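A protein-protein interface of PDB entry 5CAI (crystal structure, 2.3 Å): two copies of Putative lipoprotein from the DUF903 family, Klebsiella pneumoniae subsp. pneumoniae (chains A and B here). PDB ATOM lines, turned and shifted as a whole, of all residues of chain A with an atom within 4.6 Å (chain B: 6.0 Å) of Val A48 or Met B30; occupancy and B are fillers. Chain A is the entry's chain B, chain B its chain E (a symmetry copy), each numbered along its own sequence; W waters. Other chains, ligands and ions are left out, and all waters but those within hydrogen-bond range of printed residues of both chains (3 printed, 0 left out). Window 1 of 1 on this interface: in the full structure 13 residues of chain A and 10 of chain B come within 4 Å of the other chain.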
ATOM      1  N   MET A   8      18.916   1.589 -22.435  1.00  0.00           N
ATOM      2  CA  MET A   8      17.832   0.832 -21.844  1.00  0.00           C
ATOM      3  C   MET A   8      18.357  -0.484 -21.301  1.00  0.00           C
ATOM      4  O   MET A   8      19.043  -1.209 -22.025  1.00  0.00           O
ATOM      5  CB  MET A   8      16.791   0.594 -22.939  1.00  0.00           C
ATOM      6  CG  MET A   8      15.458   0.133 -22.434  1.00  0.00           C
ATOM      7  SD  MET A   8      14.087   0.312 -23.844  1.00  0.00           S
ATOM      8  CE  MET A   8      14.877  -0.945 -24.988  1.00  0.00           C
ATOM      9  N   HIS A   9      18.046  -0.789 -20.031  1.00  0.00           N
ATOM     10  CA  HIS A   9      18.437  -2.043 -19.388  1.00  0.00           C
ATOM     11  C   HIS A   9      17.178  -2.841 -19.188  1.00  0.00           C
ATOM     12  O   HIS A   9      16.212  -2.335 -18.604  1.00  0.00           O
ATOM     13  CB  HIS A   9      19.184  -1.814 -18.052  1.00  0.00           C
ATOM     14  CG  HIS A   9      20.461  -1.070 -18.205  1.00  0.00           C
ATOM     15  ND1 HIS A   9      21.659  -1.727 -18.404  1.00  0.00           N
ATOM     16  CD2 HIS A   9      20.684   0.262 -18.207  1.00  0.00           C
ATOM     17  CE1 HIS A   9      22.569  -0.777 -18.523  1.00  0.00           C
ATOM     18  NE2 HIS A   9      22.033   0.436 -18.393  1.00  0.00           N
ATOM     19  N   THR A  10      17.169  -4.070 -19.686  1.00  0.00           N
ATOM     20  CA  THR A  10      15.992  -4.926 -19.583  1.00  0.00           C
ATOM     21  C   THR A  10      16.108  -5.856 -18.381  1.00  0.00           C
ATOM     22  O   THR A  10      17.193  -5.999 -17.822  1.00  0.00           O
ATOM     23  CB  THR A  10      15.771  -5.708 -20.881  1.00  0.00           C
ATOM     24  OG1 THR A  10      16.892  -6.566 -21.083  1.00  0.00           O
ATOM     25  CG2 THR A  10      15.580  -4.795 -22.092  1.00  0.00           C
ATOM     26  N   ASN A  11      14.990  -6.490 -17.979  1.00  0.00           N
ATOM     27  CA  ASN A  11      15.005  -7.398 -16.832  1.00  0.00           C
ATOM     28  C   ASN A  11      15.731  -8.714 -17.153  1.00  0.00           C
ATOM     29  O   ASN A  11      16.231  -9.353 -16.220  1.00  0.00           O
ATOM     30  CB  ASN A  11      13.601  -7.638 -16.298  1.00  0.00           C
ATOM     31  CG  ASN A  11      13.053  -6.442 -15.524  1.00  0.00           C
ATOM     32  OD1 ASN A  11      13.742  -5.779 -14.740  1.00  0.00           O
ATOM     33  ND2 ASN A  11      11.793  -6.136 -15.709  1.00  0.00           N
ATOM     34  N   ILE A  43       8.922  -3.251 -27.200  1.00  0.00           N
ATOM     35  CA  ILE A  43       9.052  -4.174 -26.075  1.00  0.00           C
ATOM     36  C   ILE A  43       8.048  -3.738 -24.998  1.00  0.00           C
ATOM     37  O   ILE A  43       7.508  -2.641 -25.034  1.00  0.00           O
ATOM     38  CB  ILE A  43      10.502  -4.418 -25.539  1.00  0.00           C
ATOM     39  CG1 ILE A  43      11.144  -3.156 -24.878  1.00  0.00           C
ATOM     40  CG2 ILE A  43      11.405  -5.018 -26.641  1.00  0.00           C
ATOM     41  CD1 ILE A  43      12.451  -3.498 -24.036  1.00  0.00           C
ATOM     42  N   ASN A  44       7.760  -4.615 -24.093  1.00  0.00           N
ATOM     43  CA  ASN A  44       6.822  -4.363 -23.026  1.00  0.00           C
ATOM     44  C   ASN A  44       7.495  -3.526 -21.937  1.00  0.00           C
ATOM     45  O   ASN A  44       8.646  -3.798 -21.589  1.00  0.00           O
ATOM     46  CB  ASN A  44       6.397  -5.726 -22.486  1.00  0.00           C
ATOM     47  CG  ASN A  44       5.093  -5.690 -21.824  1.00  0.00           C
ATOM     48  OD1 ASN A  44       4.933  -5.030 -20.794  1.00  0.00           O
ATOM     49  ND2 ASN A  44       4.133  -6.365 -22.438  1.00  0.00           N
ATOM     50  N   ARG A  45       6.793  -2.523 -21.395  1.00  0.00           N
ATOM     51  CA  ARG A  45       7.301  -1.670 -20.313  1.00  0.00           C
ATOM     52  C   ARG A  45       7.743  -2.494 -19.098  1.00  0.00           C
ATOM     53  O   ARG A  45       8.777  -2.190 -18.514  1.00  0.00           O
ATOM     54  CB  ARG A  45       6.250  -0.647 -19.890  1.00  0.00           C
ATOM     55  CG  ARG A  45       6.745   0.445 -18.905  1.00  0.00           C
ATOM     56  CD  ARG A  45       5.590   1.341 -18.426  1.00  0.00           C
ATOM     57  NE  ARG A  45       5.011   2.086 -19.557  1.00  0.00           N
ATOM     58  CZ  ARG A  45       3.852   1.812 -20.154  1.00  0.00           C
ATOM     59  NH1 ARG A  45       3.086   0.824 -19.708  1.00  0.00           N
ATOM     60  NH2 ARG A  45       3.458   2.519 -21.211  1.00  0.00           N
ATOM     61  N   SER A  46       7.015  -3.560 -18.777  1.00  0.00           N
ATOM     62  CA  SER A  46       7.316  -4.439 -17.650  1.00  0.00           C
ATOM     63  C   SER A  46       8.657  -5.169 -17.810  1.00  0.00           C
ATOM     64  O   SER A  46       9.165  -5.692 -16.823  1.00  0.00           O
ATOM     65  CB  SER A  46       6.188  -5.442 -17.423  1.00  0.00           C
ATOM     66  OG  SER A  46       5.945  -6.220 -18.576  1.00  0.00           O
ATOM     67  N   ASP A  47       9.241  -5.175 -19.025  1.00  0.00           N
ATOM     68  CA  ASP A  47      10.546  -5.798 -19.273  1.00  0.00           C
ATOM     69  C   ASP A  47      11.688  -4.776 -19.199  1.00  0.00           C
ATOM     70  O   ASP A  47      12.849  -5.172 -19.202  1.00  0.00           O
ATOM     71  CB  ASP A  47      10.566  -6.563 -20.608  1.00  0.00           C
ATOM     72  CG  ASP A  47       9.638  -7.774 -20.621  1.00  0.00           C
ATOM     73  OD1 ASP A  47       9.453  -8.406 -19.543  1.00  0.00           O
ATOM     74  OD2 ASP A  47       9.069  -8.070 -21.694  1.00  0.00           O
ATOM     75  N   VAL A  48      11.364  -3.481 -19.079  1.00  0.00           N
ATOM     76  CA  VAL A  48      12.353  -2.417 -18.963  1.00  0.00           C
ATOM     77  C   VAL A  48      12.613  -2.145 -17.469  1.00  0.00           C
ATOM     78  O   VAL A  48      11.685  -1.827 -16.703  1.00  0.00           O
ATOM     79  CB  VAL A  48      11.919  -1.130 -19.709  1.00  0.00           C
ATOM     80  CG1 VAL A  48      13.052  -0.103 -19.708  1.00  0.00           C
ATOM     81  CG2 VAL A  48      11.477  -1.443 -21.138  1.00  0.00           C
ATOM     82  N   LYS A  49      13.872  -2.286 -17.066  1.00  0.00           N
ATOM     83  CA  LYS A  49      14.317  -2.071 -15.692  1.00  0.00           C
ATOM     84  C   LYS A  49      14.758  -0.606 -15.517  1.00  0.00           C
ATOM     85  O   LYS A  49      14.337   0.055 -14.573  1.00  0.00           O
ATOM     86  CB  LYS A  49      15.459  -3.054 -15.367  1.00  0.00           C
ATOM     87  CG  LYS A  49      16.000  -2.996 -13.947  1.00  0.00           C
ATOM     88  CD  LYS A  49      16.931  -4.182 -13.563  1.00  0.00           C
ATOM     89  CE  LYS A  49      18.236  -4.472 -14.309  1.00  0.00           C
ATOM     90  NZ  LYS A  49      18.743  -5.851 -14.022  1.00  0.00           N
ATOM     91  N   GLN A  50      15.612  -0.105 -16.424  1.00  0.00           N
ATOM     92  CA  GLN A  50      16.106   1.267 -16.361  1.00  0.00           C
ATOM     93  C   GLN A  50      16.201   1.864 -17.754  1.00  0.00           C
ATOM     94  O   GLN A  50      16.384   1.149 -18.730  1.00  0.00           O
ATOM     95  CB  GLN A  50      17.474   1.329 -15.652  1.00  0.00           C
ATOM     96  CG  GLN A  50      17.664   2.575 -14.787  1.00  0.00           C
ATOM     97  CD  GLN A  50      19.109   2.948 -14.536  1.00  0.00           C
ATOM     98  OE1 GLN A  50      20.014   2.102 -14.503  1.00  0.00           O
ATOM     99  NE2 GLN A  50      19.351   4.231 -14.315  1.00  0.00           N
ATOM    100  N   LEU A  51      16.108   3.178 -17.830  1.00  0.00           N
ATOM    101  CA  LEU A  51      16.197   3.948 -19.060  1.00  0.00           C
ATOM    102  C   LEU A  51      16.843   5.274 -18.712  1.00  0.00           C
ATOM    103  O   LEU A  51      16.410   5.954 -17.787  1.00  0.00           O
ATOM    104  CB  LEU A  51      14.797   4.131 -19.628  1.00  0.00           C
ATOM    105  CG  LEU A  51      14.653   4.578 -21.057  1.00  0.00           C
ATOM    106  CD1 LEU A  51      13.397   4.002 -21.588  1.00  0.00           C
ATOM    107  CD2 LEU A  51      14.456   6.037 -21.165  1.00  0.00           C
ATOM    108  N   GLN B  23       8.480  11.852 -11.321  1.00  0.00           N
ATOM    109  CA  GLN B  23       7.187  11.951 -12.002  1.00  0.00           C
ATOM    110  C   GLN B  23       7.100  10.939 -13.125  1.00  0.00           C
ATOM    111  O   GLN B  23       8.116  10.503 -13.641  1.00  0.00           O
ATOM    112  CB  GLN B  23       6.936  13.382 -12.533  1.00  0.00           C
ATOM    113  CG  GLN B  23       7.899  13.836 -13.618  1.00  0.00           C
ATOM    114  CD  GLN B  23       7.640  15.242 -14.082  1.00  0.00           C
ATOM    115  OE1 GLN B  23       6.528  15.609 -14.490  1.00  0.00           O
ATOM    116  NE2 GLN B  23       8.705  16.012 -14.160  1.00  0.00           N
ATOM    117  N   THR B  24       5.895  10.580 -13.515  1.00  0.00           N
ATOM    118  CA  THR B  24       5.657   9.645 -14.603  1.00  0.00           C
ATOM    119  C   THR B  24       6.090  10.327 -15.897  1.00  0.00           C
ATOM    120  O   THR B  24       5.682  11.456 -16.160  1.00  0.00           O
ATOM    121  CB  THR B  24       4.173   9.225 -14.603  1.00  0.00           C
ATOM    122  OG1 THR B  24       3.872   8.620 -13.347  1.00  0.00           O
ATOM    123  CG2 THR B  24       3.836   8.246 -15.716  1.00  0.00           C
ATOM    124  N   ASP B  25       6.984   9.681 -16.661  1.00  0.00           N
ATOM    125  CA  ASP B  25       7.443  10.195 -17.933  1.00  0.00           C
ATOM    126  C   ASP B  25       6.265  10.148 -18.924  1.00  0.00           C
ATOM    127  O   ASP B  25       5.571   9.129 -19.026  1.00  0.00           O
ATOM    128  CB  ASP B  25       8.656   9.402 -18.444  1.00  0.00           C
ATOM    129  CG  ASP B  25       9.236   9.969 -19.724  1.00  0.00           C
ATOM    130  OD1 ASP B  25       8.685   9.693 -20.789  1.00  0.00           O
ATOM    131  OD2 ASP B  25      10.220  10.714 -19.645  1.00  0.00           O
ATOM    132  N   ASN B  26       6.040  11.264 -19.643  1.00  0.00           N
ATOM    133  CA  ASN B  26       4.931  11.414 -20.585  1.00  0.00           C
ATOM    134  C   ASN B  26       5.049  10.522 -21.786  1.00  0.00           C
ATOM    135  O   ASN B  26       4.035  10.194 -22.387  1.00  0.00           O
ATOM    136  CB  ASN B  26       4.818  12.853 -21.055  1.00  0.00           C
ATOM    137  CG  ASN B  26       4.475  13.821 -19.953  1.00  0.00           C
ATOM    138  OD1 ASN B  26       3.800  13.461 -18.989  1.00  0.00           O
ATOM    139  ND2 ASN B  26       4.980  15.062 -20.048  1.00  0.00           N
ATOM    140  N   THR B  28       7.140   7.452 -21.908  1.00  0.00           N
ATOM    141  CA  THR B  28       7.323   6.020 -21.608  1.00  0.00           C
ATOM    142  C   THR B  28       6.408   5.457 -20.524  1.00  0.00           C
ATOM    143  O   THR B  28       6.273   4.257 -20.456  1.00  0.00           O
ATOM    144  CB  THR B  28       8.772   5.753 -21.154  1.00  0.00           C
ATOM    145  OG1 THR B  28       8.946   6.380 -19.890  1.00  0.00           O
ATOM    146  CG2 THR B  28       9.806   6.254 -22.131  1.00  0.00           C
ATOM    147  N   GLY B  29       5.891   6.286 -19.626  1.00  0.00           N
ATOM    148  CA  GLY B  29       5.050   5.782 -18.540  1.00  0.00           C
ATOM    149  C   GLY B  29       5.865   5.276 -17.366  1.00  0.00           C
ATOM    150  O   GLY B  29       5.312   4.765 -16.393  1.00  0.00           O
ATOM    151  N   MET B  30       7.191   5.412 -17.455  1.00  0.00           N
ATOM    152  CA  MET B  30       8.118   5.032 -16.387  1.00  0.00           C
ATOM    153  C   MET B  30       8.227   6.176 -15.387  1.00  0.00           C
ATOM    154  O   MET B  30       7.730   7.275 -15.650  1.00  0.00           O
ATOM    155  CB  MET B  30       9.517   4.707 -16.959  1.00  0.00           C
ATOM    156  CG  MET B  30       9.538   3.643 -18.025  1.00  0.00           C
ATOM    157  SD  MET B  30      10.186   1.997 -17.428  1.00  0.00           S
ATOM    158  CE  MET B  30      11.988   2.358 -17.081  1.00  0.00           C
ATOM    159  N   ILE B  31       8.860   5.926 -14.234  1.00  0.00           N
ATOM    160  CA  ILE B  31       9.085   6.945 -13.233  1.00  0.00           C
ATOM    161  C   ILE B  31      10.383   7.630 -13.617  1.00  0.00           C
ATOM    162  O   ILE B  31      11.428   6.996 -13.648  1.00  0.00           O
ATOM    163  CB  ILE B  31       9.107   6.381 -11.781  1.00  0.00           C
ATOM    164  CG1 ILE B  31       7.734   5.798 -11.354  1.00  0.00           C
ATOM    165  CG2 ILE B  31       9.594   7.455 -10.786  1.00  0.00           C
ATOM    166  CD1 ILE B  31       6.550   6.701 -11.540  1.00  0.00           C
ATOM    167  N   SER B  32      10.294   8.897 -13.962  1.00  0.00           N
ATOM    168  CA  SER B  32      11.425   9.743 -14.336  1.00  0.00           C
ATOM    169  C   SER B  32      11.884  10.554 -13.130  1.00  0.00           C
ATOM    170  O   SER B  32      11.058  11.072 -12.365  1.00  0.00           O
ATOM    171  CB  SER B  32      11.037  10.667 -15.486  1.00  0.00           C
ATOM    172  OG  SER B  32      12.069  11.588 -15.800  1.00  0.00           O
ATOM    173  N   GLN B  42      15.223   6.913 -15.557  1.00  0.00           N
ATOM    174  CA  GLN B  42      13.870   6.369 -15.492  1.00  0.00           C
ATOM    175  C   GLN B  42      13.893   4.971 -14.944  1.00  0.00           C
ATOM    176  O   GLN B  42      14.766   4.165 -15.313  1.00  0.00           O
ATOM    177  CB  GLN B  42      13.195   6.378 -16.867  1.00  0.00           C
ATOM    178  CG  GLN B  42      13.064   7.760 -17.465  1.00  0.00           C
ATOM    179  CD  GLN B  42      12.193   7.780 -18.671  1.00  0.00           C
ATOM    180  OE1 GLN B  42      11.253   7.020 -18.792  1.00  0.00           O
ATOM    181  NE2 GLN B  42      12.470   8.677 -19.586  1.00  0.00           N
ATOM    182  N   ILE B  43      12.950   4.680 -14.045  1.00  0.00           N
ATOM    183  CA  ILE B  43      12.799   3.337 -13.499  1.00  0.00           C
ATOM    184  C   ILE B  43      11.332   2.984 -13.566  1.00  0.00           C
ATOM    185  O   ILE B  43      10.481   3.853 -13.716  1.00  0.00           O
ATOM    186  CB  ILE B  43      13.418   3.115 -12.085  1.00  0.00           C
ATOM    187  CG1 ILE B  43      12.804   4.076 -11.047  1.00  0.00           C
ATOM    188  CG2 ILE B  43      14.977   3.198 -12.131  1.00  0.00           C
ATOM    189  CD1 ILE B  43      13.213   3.720  -9.632  1.00  0.00           C
ATOM    190  N   ASN B  44      11.041   1.718 -13.507  1.00  0.00           N
ATOM    191  CA  ASN B  44       9.689   1.208 -13.574  1.00  0.00           C
ATOM    192  C   ASN B  44       9.007   1.381 -12.232  1.00  0.00           C
ATOM    193  O   ASN B  44       9.604   1.054 -11.211  1.00  0.00           O
ATOM    194  CB  ASN B  44       9.763  -0.260 -13.962  1.00  0.00           C
ATOM    195  CG  ASN B  44       8.538  -0.732 -14.611  1.00  0.00           C
ATOM    196  OD1 ASN B  44       7.465  -0.699 -14.002  1.00  0.00           O
ATOM    197  ND2 ASN B  44       8.679  -1.163 -15.868  1.00  0.00           N
ATOM    198  N   ARG B  45       7.754   1.877 -12.221  1.00  0.00           N
ATOM    199  CA  ARG B  45       6.980   2.079 -10.986  1.00  0.00           C
ATOM    200  C   ARG B  45       6.854   0.775 -10.197  1.00  0.00           C
ATOM    201  O   ARG B  45       6.941   0.819  -8.976  1.00  0.00           O
ATOM    202  CB  ARG B  45       5.592   2.642 -11.294  1.00  0.00           C
ATOM    203  CG  ARG B  45       4.793   3.078 -10.043  1.00  0.00           C
ATOM    204  CD  ARG B  45       3.360   3.498 -10.378  1.00  0.00           C
ATOM    205  NE  ARG B  45       3.345   4.659 -11.270  1.00  0.00           N
ATOM    206  CZ  ARG B  45       3.064   4.615 -12.569  1.00  0.00           C
ATOM    207  NH1 ARG B  45       2.740   3.468 -13.147  1.00  0.00           N
ATOM    208  NH2 ARG B  45       3.116   5.715 -13.301  1.00  0.00           N
ATOM    209  N   ASP B  47       8.944  -1.431  -9.704  1.00  0.00           N
ATOM    210  CA  ASP B  47      10.190  -1.703  -8.961  1.00  0.00           C
ATOM    211  C   ASP B  47      10.356  -0.780  -7.757  1.00  0.00           C
ATOM    212  O   ASP B  47      11.233  -1.027  -6.935  1.00  0.00           O
ATOM    213  CB  ASP B  47      11.418  -1.613  -9.888  1.00  0.00           C
ATOM    214  CG  ASP B  47      11.449  -2.748 -10.911  1.00  0.00           C
ATOM    215  OD1 ASP B  47      10.954  -3.871 -10.587  1.00  0.00           O
ATOM    216  OD2 ASP B  47      11.947  -2.525 -12.025  1.00  0.00           O
HETATM  217  O   HOH W   1      13.925  -5.152 -12.082  1.00  0.00           O
HETATM  218  O   HOH W   2      10.970  -3.639 -14.559  1.00  0.00           O
HETATM  219  O   HOH W   3      12.770  -0.184 -12.653  1.00  0.00           O
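O of Arg A45 sits at hydrogen-bond distance from ND2 of Asn B44, 2.8 Å away.
NE of Arg A45 sits at hydrogen-bond distance from O of Thr B28 (2.7 Å).
The backbone carbonyl oxygen of Leu A51 sits at hydrogen-bond distance from the backbone NH of Gln B42 (2.7 Å).
ND2 of Asn B44 sits at hydrogen-bond distance from O of Val A48, at 3.2 Å.
The side-chain amide oxygen (OE1) of Gln B42 is in hydrogen-bond range of the side-chain hydroxyl (OG1) of Thr B28 (2.6 Å).
The backbone carbonyl oxygen of Gln A50 sits at hydrogen-bond distance from the backbone NH of His A9 (2.9 Å).
O of Met B30 lies within hydrogen-bond range of N of Asp B25, at 2.7 Å.
OG1 of Thr B28 sits at hydrogen-bond distance from N of Met B30 (3.2 Å).
The backbone NH (N) of Thr B28 lies within hydrogen-bond range of the side-chain carboxylate (OD1) of Asp B25 (2.9 Å).
The side-chain hydroxyl (OG) of Ser A46 lies within hydrogen-bond range of the side-chain amide oxygen (OD1) of Asn A44 (2.7 Å).
CA of Gly B29 touches NE of Arg A45, 3.8 Å away.
Ser A46 touches Asn B44.
Val A48 touches Met B30 (CG1 to CE, 3.8 Å).
O of Lys A49 touches CA of Ile B43, at 3.8 Å.
O of Lys A49 touches N of Asn B44, 3.8 Å away.
Gln A50 touches Gln B42.
Gln A50 touches Ile B43.
Of the printed residues of chain B, Val A48 touches Met B30 (3.8 Å) and Asn B44 (3.2 Å).
Of the printed residues of chain B, Lys A49 touches Ile B43 and Asn B44.
Printed residues of chain A within 4 Å of Met B30: Val A48 (3.8 Å).
Of the printed residues of chain A, Ile B43 touches Lys A49 (3.8 Å) and Gln A50 (3.8 Å).
The nearest printed residue of chain A that does not touch Met B30 is Arg A45 (4.1 Å).
Of the 13 printed residues of chain A, 6 touch a printed residue of chain B.
Hydrophobic or aromatic side chains of chain A within 4 Å of the printed part of chain B: Val A48 and Leu A51.
Of the 14 printed residues of chain B, 6 touch a printed residue of chain A.
Hydrophobic or aromatic side chains of chain B within 4 Å of the printed part of chain A: Met B30 and Ile B43.
Among the printed residues, 11 pairs touch across the chains.
Among the printed residues, no Asp or Glu carboxylate lies within 4 Å of a Lys or Arg side-chain nitrogen of the other chain.
Arg A45 touches Asn B44, but with the chains exchanged Asn A44 does not touch Arg B45 (11.0 Å).
4 positions are printed for both chains.
Of the 11 pairs that touch across the chains among the printed residues, none has its exchanged pair printed and touching as well.
Water W3 lies within hydrogen-bond range of O of Lys A49 (2.5 Å), OD2 of Asp B47 (2.6 Å) and N of Asn B44 (2.7 Å).
Water W1 bridges the side-chain amide oxygen of Asn A11 and the side-chain carboxylate of Asp B47.
Water W2 lies within hydrogen-bond range of the side-chain amide nitrogen (ND2) of Asn A11 (2.9 Å), the backbone carbonyl oxygen (O) of Val A48 (2.9 Å) and the side-chain carboxylate (OD2) of Asp B47 (2.9 Å).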
